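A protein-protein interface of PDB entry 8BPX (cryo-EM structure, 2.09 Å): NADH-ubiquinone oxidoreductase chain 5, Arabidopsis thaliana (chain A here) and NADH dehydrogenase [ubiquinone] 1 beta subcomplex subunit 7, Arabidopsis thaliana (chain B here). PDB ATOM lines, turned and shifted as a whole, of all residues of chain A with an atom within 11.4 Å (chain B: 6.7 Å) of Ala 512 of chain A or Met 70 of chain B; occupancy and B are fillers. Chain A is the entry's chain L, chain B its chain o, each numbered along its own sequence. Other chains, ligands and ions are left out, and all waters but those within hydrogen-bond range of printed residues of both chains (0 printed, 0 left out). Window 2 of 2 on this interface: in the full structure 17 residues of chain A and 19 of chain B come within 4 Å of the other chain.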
ATOM      1  N   LEU A 405      18.399 -12.137 -17.591  1.00  0.00           N
ATOM      2  CA  LEU A 405      19.782 -12.608 -17.596  1.00  0.00           C
ATOM      3  C   LEU A 405      19.976 -13.784 -16.635  1.00  0.00           C
ATOM      4  O   LEU A 405      20.668 -14.756 -16.963  1.00  0.00           O
ATOM      5  CB  LEU A 405      20.725 -11.454 -17.262  1.00  0.00           C
ATOM      6  CG  LEU A 405      21.190 -10.623 -18.466  1.00  0.00           C
ATOM      7  CD1 LEU A 405      22.272  -9.642 -18.066  1.00  0.00           C
ATOM      8  CD2 LEU A 405      21.662 -11.501 -19.620  1.00  0.00           C
ATOM      9  N   GLU A 406      19.392 -13.744 -15.457  1.00  0.00           N
ATOM     10  CA  GLU A 406      19.423 -14.837 -14.476  1.00  0.00           C
ATOM     11  C   GLU A 406      18.760 -16.096 -15.001  1.00  0.00           C
ATOM     12  O   GLU A 406      19.331 -17.137 -14.758  1.00  0.00           O
ATOM     13  CB  GLU A 406      18.644 -14.373 -13.234  1.00  0.00           C
ATOM     14  CG  GLU A 406      19.474 -13.625 -12.233  1.00  0.00           C
ATOM     15  CD  GLU A 406      18.605 -12.699 -11.414  1.00  0.00           C
ATOM     16  OE1 GLU A 406      17.595 -13.172 -10.873  1.00  0.00           O
ATOM     17  OE2 GLU A 406      18.918 -11.509 -11.354  1.00  0.00           O
ATOM     18  N   LEU A 407      17.616 -15.955 -15.719  1.00  0.00           N
ATOM     19  CA  LEU A 407      16.955 -17.103 -16.329  1.00  0.00           C
ATOM     20  C   LEU A 407      17.820 -17.715 -17.418  1.00  0.00           C
ATOM     21  O   LEU A 407      17.899 -18.942 -17.543  1.00  0.00           O
ATOM     22  CB  LEU A 407      15.596 -16.690 -16.896  1.00  0.00           C
ATOM     23  CG  LEU A 407      14.463 -16.390 -15.917  1.00  0.00           C
ATOM     24  CD1 LEU A 407      13.334 -15.657 -16.617  1.00  0.00           C
ATOM     25  CD2 LEU A 407      13.959 -17.672 -15.275  1.00  0.00           C
ATOM     26  N   ALA A 408      18.542 -16.895 -18.166  1.00  0.00           N
ATOM     27  CA  ALA A 408      19.415 -17.435 -19.220  1.00  0.00           C
ATOM     28  C   ALA A 408      20.541 -18.213 -18.569  1.00  0.00           C
ATOM     29  O   ALA A 408      20.928 -19.211 -19.073  1.00  0.00           O
ATOM     30  CB  ALA A 408      19.957 -16.342 -20.068  1.00  0.00           C
ATOM     31  N   TYR A 409      21.052 -17.639 -17.488  1.00  0.00           N
ATOM     32  CA  TYR A 409      22.081 -18.375 -16.765  1.00  0.00           C
ATOM     33  C   TYR A 409      21.563 -19.733 -16.305  1.00  0.00           C
ATOM     34  O   TYR A 409      22.298 -20.726 -16.314  1.00  0.00           O
ATOM     35  CB  TYR A 409      22.570 -17.566 -15.570  1.00  0.00           C
ATOM     36  CG  TYR A 409      23.523 -18.339 -14.701  1.00  0.00           C
ATOM     37  CD1 TYR A 409      24.847 -18.502 -15.073  1.00  0.00           C
ATOM     38  CD2 TYR A 409      23.091 -18.942 -13.525  1.00  0.00           C
ATOM     39  CE1 TYR A 409      25.722 -19.220 -14.291  1.00  0.00           C
ATOM     40  CE2 TYR A 409      23.961 -19.664 -12.737  1.00  0.00           C
ATOM     41  CZ  TYR A 409      25.273 -19.800 -13.125  1.00  0.00           C
ATOM     42  OH  TYR A 409      26.142 -20.516 -12.344  1.00  0.00           O
ATOM     43  N   THR A 410      20.300 -19.792 -15.892  1.00  0.00           N
ATOM     44  CA  THR A 410      19.723 -21.019 -15.360  1.00  0.00           C
ATOM     45  C   THR A 410      19.340 -22.024 -16.445  1.00  0.00           C
ATOM     46  O   THR A 410      19.130 -23.200 -16.136  1.00  0.00           O
ATOM     47  CB  THR A 410      18.514 -20.660 -14.491  1.00  0.00           C
ATOM     48  OG1 THR A 410      18.876 -19.572 -13.635  1.00  0.00           O
ATOM     49  CG2 THR A 410      18.077 -21.825 -13.633  1.00  0.00           C
ATOM     50  N   LYS A 411      19.269 -21.608 -17.706  1.00  0.00           N
ATOM     51  CA  LYS A 411      18.971 -22.540 -18.792  1.00  0.00           C
ATOM     52  C   LYS A 411      20.233 -23.325 -19.123  1.00  0.00           C
ATOM     53  O   LYS A 411      21.133 -22.827 -19.804  1.00  0.00           O
ATOM     54  CB  LYS A 411      18.433 -21.797 -20.008  1.00  0.00           C
ATOM     55  CG  LYS A 411      17.886 -22.702 -21.089  1.00  0.00           C
ATOM     56  CD  LYS A 411      16.374 -22.791 -21.030  1.00  0.00           C
ATOM     57  CE  LYS A 411      15.836 -23.790 -22.040  1.00  0.00           C
ATOM     58  NZ  LYS A 411      14.803 -24.685 -21.463  1.00  0.00           N
ATOM     59  N   TYR A 412      20.304 -24.567 -18.647  1.00  0.00           N
ATOM     60  CA  TYR A 412      21.502 -25.391 -18.818  1.00  0.00           C
ATOM     61  C   TYR A 412      21.430 -26.132 -20.154  1.00  0.00           C
ATOM     62  O   TYR A 412      21.281 -27.351 -20.232  1.00  0.00           O
ATOM     63  CB  TYR A 412      21.672 -26.336 -17.637  1.00  0.00           C
ATOM     64  CG  TYR A 412      22.383 -25.688 -16.474  1.00  0.00           C
ATOM     65  CD1 TYR A 412      21.690 -24.914 -15.557  1.00  0.00           C
ATOM     66  CD2 TYR A 412      23.751 -25.822 -16.314  1.00  0.00           C
ATOM     67  CE1 TYR A 412      22.337 -24.308 -14.503  1.00  0.00           C
ATOM     68  CE2 TYR A 412      24.408 -25.218 -15.269  1.00  0.00           C
ATOM     69  CZ  TYR A 412      23.695 -24.461 -14.367  1.00  0.00           C
ATOM     70  OH  TYR A 412      24.348 -23.858 -13.321  1.00  0.00           O
ATOM     71  N   LEU A 488       6.342 -15.356  -8.245  1.00  0.00           N
ATOM     72  CA  LEU A 488       6.355 -16.813  -8.165  1.00  0.00           C
ATOM     73  C   LEU A 488       4.952 -17.377  -7.981  1.00  0.00           C
ATOM     74  O   LEU A 488       4.276 -17.082  -6.994  1.00  0.00           O
ATOM     75  CB  LEU A 488       7.258 -17.257  -7.012  1.00  0.00           C
ATOM     76  CG  LEU A 488       8.186 -18.441  -7.279  1.00  0.00           C
ATOM     77  CD1 LEU A 488       9.125 -18.132  -8.427  1.00  0.00           C
ATOM     78  CD2 LEU A 488       8.963 -18.823  -6.029  1.00  0.00           C
ATOM     79  N   GLU A 504       9.889 -25.035 -16.628  1.00  0.00           N
ATOM     80  CA  GLU A 504       9.789 -24.057 -15.513  1.00  0.00           C
ATOM     81  C   GLU A 504      11.152 -23.909 -14.799  1.00  0.00           C
ATOM     82  O   GLU A 504      11.651 -24.870 -14.269  1.00  0.00           O
ATOM     83  CB  GLU A 504       8.564 -24.369 -14.627  1.00  0.00           C
ATOM     84  CG  GLU A 504       7.259 -23.740 -15.061  1.00  0.00           C
ATOM     85  CD  GLU A 504       7.121 -22.224 -15.141  1.00  0.00           C
ATOM     86  OE1 GLU A 504       8.125 -21.502 -15.017  1.00  0.00           O
ATOM     87  OE2 GLU A 504       5.990 -21.765 -15.339  1.00  0.00           O
ATOM     88  N   ILE A 505      11.724 -22.736 -14.819  1.00  0.00           N
ATOM     89  CA  ILE A 505      13.055 -22.431 -14.229  1.00  0.00           C
ATOM     90  C   ILE A 505      13.039 -21.189 -13.333  1.00  0.00           C
ATOM     91  O   ILE A 505      14.098 -20.868 -12.853  1.00  0.00           O
ATOM     92  CB  ILE A 505      14.124 -22.234 -15.348  1.00  0.00           C
ATOM     93  CG1 ILE A 505      13.776 -21.087 -16.297  1.00  0.00           C
ATOM     94  CG2 ILE A 505      14.409 -23.522 -16.114  1.00  0.00           C
ATOM     95  CD1 ILE A 505      14.874 -20.767 -17.278  1.00  0.00           C
ATOM     96  N   LEU A 506      11.933 -20.522 -13.114  1.00  0.00           N
ATOM     97  CA  LEU A 506      11.948 -19.254 -12.347  1.00  0.00           C
ATOM     98  C   LEU A 506      12.449 -19.446 -10.872  1.00  0.00           C
ATOM     99  O   LEU A 506      13.311 -18.666 -10.487  1.00  0.00           O
ATOM    100  CB  LEU A 506      10.603 -18.580 -12.409  1.00  0.00           C
ATOM    101  CG  LEU A 506      10.532 -17.182 -11.794  1.00  0.00           C
ATOM    102  CD1 LEU A 506      11.373 -16.173 -12.565  1.00  0.00           C
ATOM    103  CD2 LEU A 506       9.095 -16.712 -11.675  1.00  0.00           C
ATOM    104  N   ALA A 507      11.987 -20.442 -10.130  1.00  0.00           N
ATOM    105  CA  ALA A 507      12.444 -20.748  -8.737  1.00  0.00           C
ATOM    106  C   ALA A 507      13.952 -20.950  -8.692  1.00  0.00           C
ATOM    107  O   ALA A 507      14.577 -20.212  -7.982  1.00  0.00           O
ATOM    108  CB  ALA A 507      11.711 -21.946  -8.196  1.00  0.00           C
ATOM    109  N   GLU A 508      14.481 -21.839  -9.521  1.00  0.00           N
ATOM    110  CA  GLU A 508      15.919 -22.151  -9.582  1.00  0.00           C
ATOM    111  C   GLU A 508      16.731 -20.890  -9.935  1.00  0.00           C
ATOM    112  O   GLU A 508      17.847 -20.815  -9.474  1.00  0.00           O
ATOM    113  CB  GLU A 508      16.174 -23.363 -10.503  1.00  0.00           C
ATOM    114  CG  GLU A 508      15.358 -24.593 -10.206  1.00  0.00           C
ATOM    115  CD  GLU A 508      14.116 -24.773 -11.061  1.00  0.00           C
ATOM    116  OE1 GLU A 508      13.338 -23.827 -11.183  1.00  0.00           O
ATOM    117  OE2 GLU A 508      13.937 -25.858 -11.591  1.00  0.00           O
ATOM    118  N   SER A 509      16.207 -19.984 -10.744  1.00  0.00           N
ATOM    119  CA  SER A 509      16.903 -18.706 -11.032  1.00  0.00           C
ATOM    120  C   SER A 509      16.859 -17.761  -9.807  1.00  0.00           C
ATOM    121  O   SER A 509      17.794 -17.035  -9.607  1.00  0.00           O
ATOM    122  CB  SER A 509      16.374 -18.039 -12.270  1.00  0.00           C
ATOM    123  OG  SER A 509      15.283 -17.175 -12.020  1.00  0.00           O
ATOM    124  N   GLU A 510      15.774 -17.736  -9.087  1.00  0.00           N
ATOM    125  CA  GLU A 510      15.771 -16.901  -7.890  1.00  0.00           C
ATOM    126  C   GLU A 510      16.470 -17.560  -6.692  1.00  0.00           C
ATOM    127  O   GLU A 510      16.784 -16.841  -5.786  1.00  0.00           O
ATOM    128  CB  GLU A 510      14.357 -16.441  -7.566  1.00  0.00           C
ATOM    129  CG  GLU A 510      13.407 -17.400  -6.930  1.00  0.00           C
ATOM    130  CD  GLU A 510      12.381 -16.547  -6.214  1.00  0.00           C
ATOM    131  OE1 GLU A 510      12.759 -15.504  -5.656  1.00  0.00           O
ATOM    132  OE2 GLU A 510      11.209 -16.912  -6.222  1.00  0.00           O
ATOM    133  N   PHE A 511      16.808 -18.833  -6.757  1.00  0.00           N
ATOM    134  CA  PHE A 511      17.233 -19.464  -5.510  1.00  0.00           C
ATOM    135  C   PHE A 511      18.544 -20.237  -5.629  1.00  0.00           C
ATOM    136  O   PHE A 511      19.319 -20.289  -4.670  1.00  0.00           O
ATOM    137  CB  PHE A 511      16.128 -20.388  -4.990  1.00  0.00           C
ATOM    138  CG  PHE A 511      14.932 -19.656  -4.454  1.00  0.00           C
ATOM    139  CD1 PHE A 511      15.086 -18.497  -3.715  1.00  0.00           C
ATOM    140  CD2 PHE A 511      13.649 -20.117  -4.703  1.00  0.00           C
ATOM    141  CE1 PHE A 511      13.987 -17.817  -3.232  1.00  0.00           C
ATOM    142  CE2 PHE A 511      12.546 -19.443  -4.219  1.00  0.00           C
ATOM    143  CZ  PHE A 511      12.716 -18.291  -3.484  1.00  0.00           C
ATOM    144  N   ALA A 512      18.803 -20.851  -6.780  1.00  0.00           N
ATOM    145  CA  ALA A 512      19.979 -21.690  -6.965  1.00  0.00           C
ATOM    146  C   ALA A 512      21.135 -20.965  -7.642  1.00  0.00           C
ATOM    147  O   ALA A 512      22.147 -21.594  -7.956  1.00  0.00           O
ATOM    148  CB  ALA A 512      19.617 -22.943  -7.764  1.00  0.00           C
ATOM    149  N   ALA A 513      21.032 -19.656  -7.856  1.00  0.00           N
ATOM    150  CA  ALA A 513      22.113 -18.966  -8.589  1.00  0.00           C
ATOM    151  C   ALA A 513      23.124 -18.401  -7.599  1.00  0.00           C
ATOM    152  O   ALA A 513      22.729 -17.782  -6.630  1.00  0.00           O
ATOM    153  CB  ALA A 513      21.609 -17.872  -9.462  1.00  0.00           C
ATOM    154  N   PRO A 514      24.411 -18.474  -7.915  1.00  0.00           N
ATOM    155  CA  PRO A 514      25.404 -17.858  -7.071  1.00  0.00           C
ATOM    156  C   PRO A 514      25.078 -16.367  -7.010  1.00  0.00           C
ATOM    157  O   PRO A 514      24.714 -15.797  -8.037  1.00  0.00           O
ATOM    158  CB  PRO A 514      26.669 -18.166  -7.863  1.00  0.00           C
ATOM    159  CG  PRO A 514      26.364 -19.322  -8.757  1.00  0.00           C
ATOM    160  CD  PRO A 514      24.920 -19.125  -9.121  1.00  0.00           C
ATOM    161  N   THR A 515      25.178 -15.750  -5.846  1.00  0.00           N
ATOM    162  CA  THR A 515      24.964 -14.293  -5.681  1.00  0.00           C
ATOM    163  C   THR A 515      25.744 -13.442  -6.702  1.00  0.00           C
ATOM    164  O   THR A 515      25.233 -12.402  -7.056  1.00  0.00           O
ATOM    165  CB  THR A 515      25.398 -13.817  -4.279  1.00  0.00           C
ATOM    166  OG1 THR A 515      26.705 -14.332  -4.037  1.00  0.00           O
ATOM    167  CG2 THR A 515      24.434 -14.224  -3.188  1.00  0.00           C
ATOM    168  N   ILE A 516      26.948 -13.849  -7.118  1.00  0.00           N
ATOM    169  CA  ILE A 516      27.721 -13.073  -8.122  1.00  0.00           C
ATOM    170  C   ILE A 516      26.885 -12.865  -9.386  1.00  0.00           C
ATOM    171  O   ILE A 516      26.888 -11.734  -9.849  1.00  0.00           O
ATOM    172  CB  ILE A 516      29.081 -13.734  -8.495  1.00  0.00           C
ATOM    173  CG1 ILE A 516      30.016 -12.744  -9.190  1.00  0.00           C
ATOM    174  CG2 ILE A 516      28.957 -15.021  -9.283  1.00  0.00           C
ATOM    175  CD1 ILE A 516      30.163 -11.436  -8.471  1.00  0.00           C
ATOM    176  N   ILE A 517      26.264 -13.919  -9.907  1.00  0.00           N
ATOM    177  CA  ILE A 517      25.533 -13.908 -11.187  1.00  0.00           C
ATOM    178  C   ILE A 517      24.575 -12.742 -11.192  1.00  0.00           C
ATOM    179  O   ILE A 517      24.461 -12.098 -12.203  1.00  0.00           O
ATOM    180  CB  ILE A 517      24.910 -15.304 -11.478  1.00  0.00           C
ATOM    181  CG1 ILE A 517      25.961 -16.375 -11.776  1.00  0.00           C
ATOM    182  CG2 ILE A 517      23.878 -15.230 -12.598  1.00  0.00           C
ATOM    183  CD1 ILE A 517      26.905 -16.035 -12.894  1.00  0.00           C
ATOM    184  N   LYS A 518      24.022 -12.427 -10.034  1.00  0.00           N
ATOM    185  CA  LYS A 518      23.006 -11.375  -9.958  1.00  0.00           C
ATOM    186  C   LYS A 518      23.645  -9.987 -10.041  1.00  0.00           C
ATOM    187  O   LYS A 518      22.932  -9.074 -10.308  1.00  0.00           O
ATOM    188  CB  LYS A 518      22.184 -11.687  -8.707  1.00  0.00           C
ATOM    189  CG  LYS A 518      21.909 -13.176  -8.520  1.00  0.00           C
ATOM    190  CD  LYS A 518      21.326 -13.533  -7.168  1.00  0.00           C
ATOM    191  CE  LYS A 518      19.844 -13.830  -7.213  1.00  0.00           C
ATOM    192  NZ  LYS A 518      19.549 -15.077  -7.957  1.00  0.00           N
ATOM    193  N   TYR B  63      11.957 -22.432  -2.029  1.00  0.00           N
ATOM    194  CA  TYR B  63      13.394 -22.452  -1.797  1.00  0.00           C
ATOM    195  C   TYR B  63      13.834 -23.791  -1.222  1.00  0.00           C
ATOM    196  O   TYR B  63      14.864 -24.333  -1.630  1.00  0.00           O
ATOM    197  CB  TYR B  63      13.786 -21.297  -0.874  1.00  0.00           C
ATOM    198  CG  TYR B  63      15.175 -21.391  -0.282  1.00  0.00           C
ATOM    199  CD1 TYR B  63      15.397 -22.059   0.917  1.00  0.00           C
ATOM    200  CD2 TYR B  63      16.264 -20.802  -0.911  1.00  0.00           C
ATOM    201  CE1 TYR B  63      16.652 -22.147   1.462  1.00  0.00           C
ATOM    202  CE2 TYR B  63      17.529 -20.883  -0.369  1.00  0.00           C
ATOM    203  CZ  TYR B  63      17.716 -21.561   0.816  1.00  0.00           C
ATOM    204  OH  TYR B  63      18.970 -21.655   1.366  1.00  0.00           O
ATOM    205  N   LEU B  65      12.364 -26.689  -1.666  1.00  0.00           N
ATOM    206  CA  LEU B  65      12.308 -27.659  -2.761  1.00  0.00           C
ATOM    207  C   LEU B  65      13.581 -27.608  -3.604  1.00  0.00           C
ATOM    208  O   LEU B  65      14.210 -28.645  -3.891  1.00  0.00           O
ATOM    209  CB  LEU B  65      11.079 -27.394  -3.634  1.00  0.00           C
ATOM    210  CG  LEU B  65       9.746 -28.060  -3.280  1.00  0.00           C
ATOM    211  CD1 LEU B  65       8.841 -28.139  -4.500  1.00  0.00           C
ATOM    212  CD2 LEU B  65       9.959 -29.442  -2.687  1.00  0.00           C
ATOM    213  N   VAL B  66      13.984 -26.397  -3.994  1.00  0.00           N
ATOM    214  CA  VAL B  66      15.192 -26.243  -4.800  1.00  0.00           C
ATOM    215  C   VAL B  66      16.417 -26.731  -4.037  1.00  0.00           C
ATOM    216  O   VAL B  66      17.310 -27.361  -4.613  1.00  0.00           O
ATOM    217  CB  VAL B  66      15.357 -24.784  -5.262  1.00  0.00           C
ATOM    218  CG1 VAL B  66      16.554 -24.660  -6.175  1.00  0.00           C
ATOM    219  CG2 VAL B  66      14.116 -24.324  -5.989  1.00  0.00           C
ATOM    220  N   MET B  67      16.486 -26.441  -2.739  1.00  0.00           N
ATOM    221  CA  MET B  67      17.639 -26.870  -1.953  1.00  0.00           C
ATOM    222  C   MET B  67      17.735 -28.388  -1.887  1.00  0.00           C
ATOM    223  O   MET B  67      18.833 -28.947  -1.975  1.00  0.00           O
ATOM    224  CB  MET B  67      17.578 -26.270  -0.551  1.00  0.00           C
ATOM    225  CG  MET B  67      17.883 -24.794  -0.514  1.00  0.00           C
ATOM    226  SD  MET B  67      19.363 -24.387  -1.453  1.00  0.00           S
ATOM    227  CE  MET B  67      18.681 -23.265  -2.671  1.00  0.00           C
ATOM    228  N   GLU B  68      16.602 -29.074  -1.728  1.00  0.00           N
ATOM    229  CA  GLU B  68      16.642 -30.533  -1.714  1.00  0.00           C
ATOM    230  C   GLU B  68      17.136 -31.076  -3.047  1.00  0.00           C
ATOM    231  O   GLU B  68      17.934 -32.020  -3.084  1.00  0.00           O
ATOM    232  CB  GLU B  68      15.271 -31.120  -1.379  1.00  0.00           C
ATOM    233  CG  GLU B  68      14.649 -30.576  -0.115  1.00  0.00           C
ATOM    234  CD  GLU B  68      13.179 -30.923   0.001  1.00  0.00           C
ATOM    235  OE1 GLU B  68      12.381 -30.422  -0.818  1.00  0.00           O
ATOM    236  OE2 GLU B  68      12.822 -31.699   0.912  1.00  0.00           O
ATOM    237  N   ARG B  69      16.704 -30.569  -4.175  1.00  0.00           N
ATOM    238  CA  ARG B  69      17.200 -30.972  -5.514  1.00  0.00           C
ATOM    239  C   ARG B  69      18.679 -30.573  -5.702  1.00  0.00           C
ATOM    240  O   ARG B  69      19.371 -31.225  -6.439  1.00  0.00           O
ATOM    241  CB  ARG B  69      16.161 -30.452  -6.524  1.00  0.00           C
ATOM    242  CG  ARG B  69      14.864 -31.219  -6.676  1.00  0.00           C
ATOM    243  CD  ARG B  69      13.916 -30.426  -7.559  1.00  0.00           C
ATOM    244  NE  ARG B  69      14.553 -29.953  -8.776  1.00  0.00           N
ATOM    245  CZ  ARG B  69      14.384 -28.755  -9.314  1.00  0.00           C
ATOM    246  NH1 ARG B  69      13.560 -27.887  -8.764  1.00  0.00           N
ATOM    247  NH2 ARG B  69      15.031 -28.433 -10.416  1.00  0.00           N
ATOM    248  N   MET B  70      19.153 -29.539  -5.033  1.00  0.00           N
ATOM    249  CA  MET B  70      20.580 -29.226  -5.081  1.00  0.00           C
ATOM    250  C   MET B  70      21.407 -30.232  -4.282  1.00  0.00           C
ATOM    251  O   MET B  70      22.468 -30.671  -4.738  1.00  0.00           O
ATOM    252  CB  MET B  70      20.823 -27.805  -4.575  1.00  0.00           C
ATOM    253  CG  MET B  70      20.253 -26.722  -5.469  1.00  0.00           C
ATOM    254  SD  MET B  70      20.753 -25.054  -5.010  1.00  0.00           S
ATOM    255  CE  MET B  70      22.443 -25.029  -5.586  1.00  0.00           C
ATOM    256  N   LEU B  71      20.943 -30.607  -3.083  1.00  0.00           N
ATOM    257  CA  LEU B  71      21.657 -31.625  -2.310  1.00  0.00           C
ATOM    258  C   LEU B  71      21.632 -32.977  -3.011  1.00  0.00           C
ATOM    259  O   LEU B  71      22.625 -33.715  -2.985  1.00  0.00           O
ATOM    260  CB  LEU B  71      21.090 -31.751  -0.894  1.00  0.00           C
ATOM    261  CG  LEU B  71      21.609 -30.770   0.163  1.00  0.00           C
ATOM    262  CD1 LEU B  71      20.663 -29.605   0.397  1.00  0.00           C
ATOM    263  CD2 LEU B  71      21.890 -31.500   1.460  1.00  0.00           C
ATOM    264  N   ALA B  72      20.507 -33.323  -3.638  1.00  0.00           N
ATOM    265  CA  ALA B  72      20.444 -34.567  -4.396  1.00  0.00           C
ATOM    266  C   ALA B  72      21.479 -34.580  -5.517  1.00  0.00           C
ATOM    267  O   ALA B  72      22.192 -35.573  -5.713  1.00  0.00           O
ATOM    268  CB  ALA B  72      19.038 -34.763  -4.956  1.00  0.00           C
ATOM    269  N   MET B  73      21.587 -33.473  -6.260  1.00  0.00           N
ATOM    270  CA  MET B  73      22.592 -33.418  -7.318  1.00  0.00           C
ATOM    271  C   MET B  73      24.005 -33.427  -6.748  1.00  0.00           C
ATOM    272  O   MET B  73      24.917 -33.966  -7.378  1.00  0.00           O
ATOM    273  CB  MET B  73      22.379 -32.190  -8.199  1.00  0.00           C
ATOM    274  CG  MET B  73      23.355 -32.072  -9.362  1.00  0.00           C
ATOM    275  SD  MET B  73      23.483 -33.564 -10.371  1.00  0.00           S
ATOM    276  CE  MET B  73      22.014 -33.446 -11.381  1.00  0.00           C
ATOM    277  N   LYS B  74      24.209 -32.833  -5.572  1.00  0.00           N
ATOM    278  CA  LYS B  74      25.513 -32.908  -4.919  1.00  0.00           C
ATOM    279  C   LYS B  74      25.895 -34.358  -4.636  1.00  0.00           C
ATOM    280  O   LYS B  74      27.025 -34.780  -4.905  1.00  0.00           O
ATOM    281  CB  LYS B  74      25.494 -32.097  -3.624  1.00  0.00           C
ATOM    282  CG  LYS B  74      26.815 -32.043  -2.895  1.00  0.00           C
ATOM    283  CD  LYS B  74      26.718 -31.177  -1.650  1.00  0.00           C
ATOM    284  CE  LYS B  74      28.031 -31.129  -0.887  1.00  0.00           C
ATOM    285  NZ  LYS B  74      27.921 -30.280   0.328  1.00  0.00           N
ATOM    286  N   LYS B  75      24.988 -35.192  -4.087  1.00  0.00           N
ATOM    287  CA  LYS B  75      25.217 -36.670  -3.923  1.00  0.00           C
ATOM    288  C   LYS B  75      25.537 -37.439  -5.218  1.00  0.00           C
ATOM    289  O   LYS B  75      26.566 -38.076  -5.226  1.00  0.00           O
ATOM    290  CB  LYS B  75      24.112 -37.374  -3.121  1.00  0.00           C
ATOM    291  CG  LYS B  75      24.333 -37.443  -1.623  1.00  0.00           C
ATOM    292  CD  LYS B  75      23.333 -38.315  -0.891  1.00  0.00           C
ATOM    293  CE  LYS B  75      23.264 -39.727  -1.435  1.00  0.00           C
ATOM    294  NZ  LYS B  75      24.600 -40.366  -1.483  1.00  0.00           N
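Hydrophobic or aromatic side chains of chain B that line the printed part of chain A: Tyr 63, Val 66, Met 67 and Met 70. Of the 24 printed residues of chain A, 3 touch a printed residue of chain B. Printed residues of chain A that touch a printed residue of chain B: Glu 508, Phe 511 and Ala 512. Along chain A the printed residues that touch a printed residue of chain B span positions 508 to 512.
Ala 512 of chain A touches two residues of chain B. Met 70 of chain B touches just one residue of chain A: Ala 512. Val 66 of chain B touches just one residue of chain A: Ala 512. Leu 71 of chain B touches none of the printed residues of chain A. Met 73 of chain B touches none of the printed residues of chain A. Of the printed residues of chain A, Tyr 63 of chain B touches Phe 511 (3.7 Å). Of the printed residues of chain B, Phe 511 of chain A touches Tyr 63 and Met 67. Of the printed residues of chain B, Glu 508 of chain A touches Arg 69 (3.0 Å).
Tyr 63 of chain B touches Phe 511 of chain A (CA to CD2, 3.7 Å). CE of Met 67 of chain B touches O of Phe 511 of chain A (3.6 Å). Ala 512 of chain A touches Val 66 of chain B. SD of Met 70 of chain B touches CB of Ala 512 of chain A, at 3.7 Å.
The guanidinium group of Arg 69 of chain B lies within salt-bridge range of the side-chain carboxylate of Glu 508 of chain A, 3.0 Å away.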
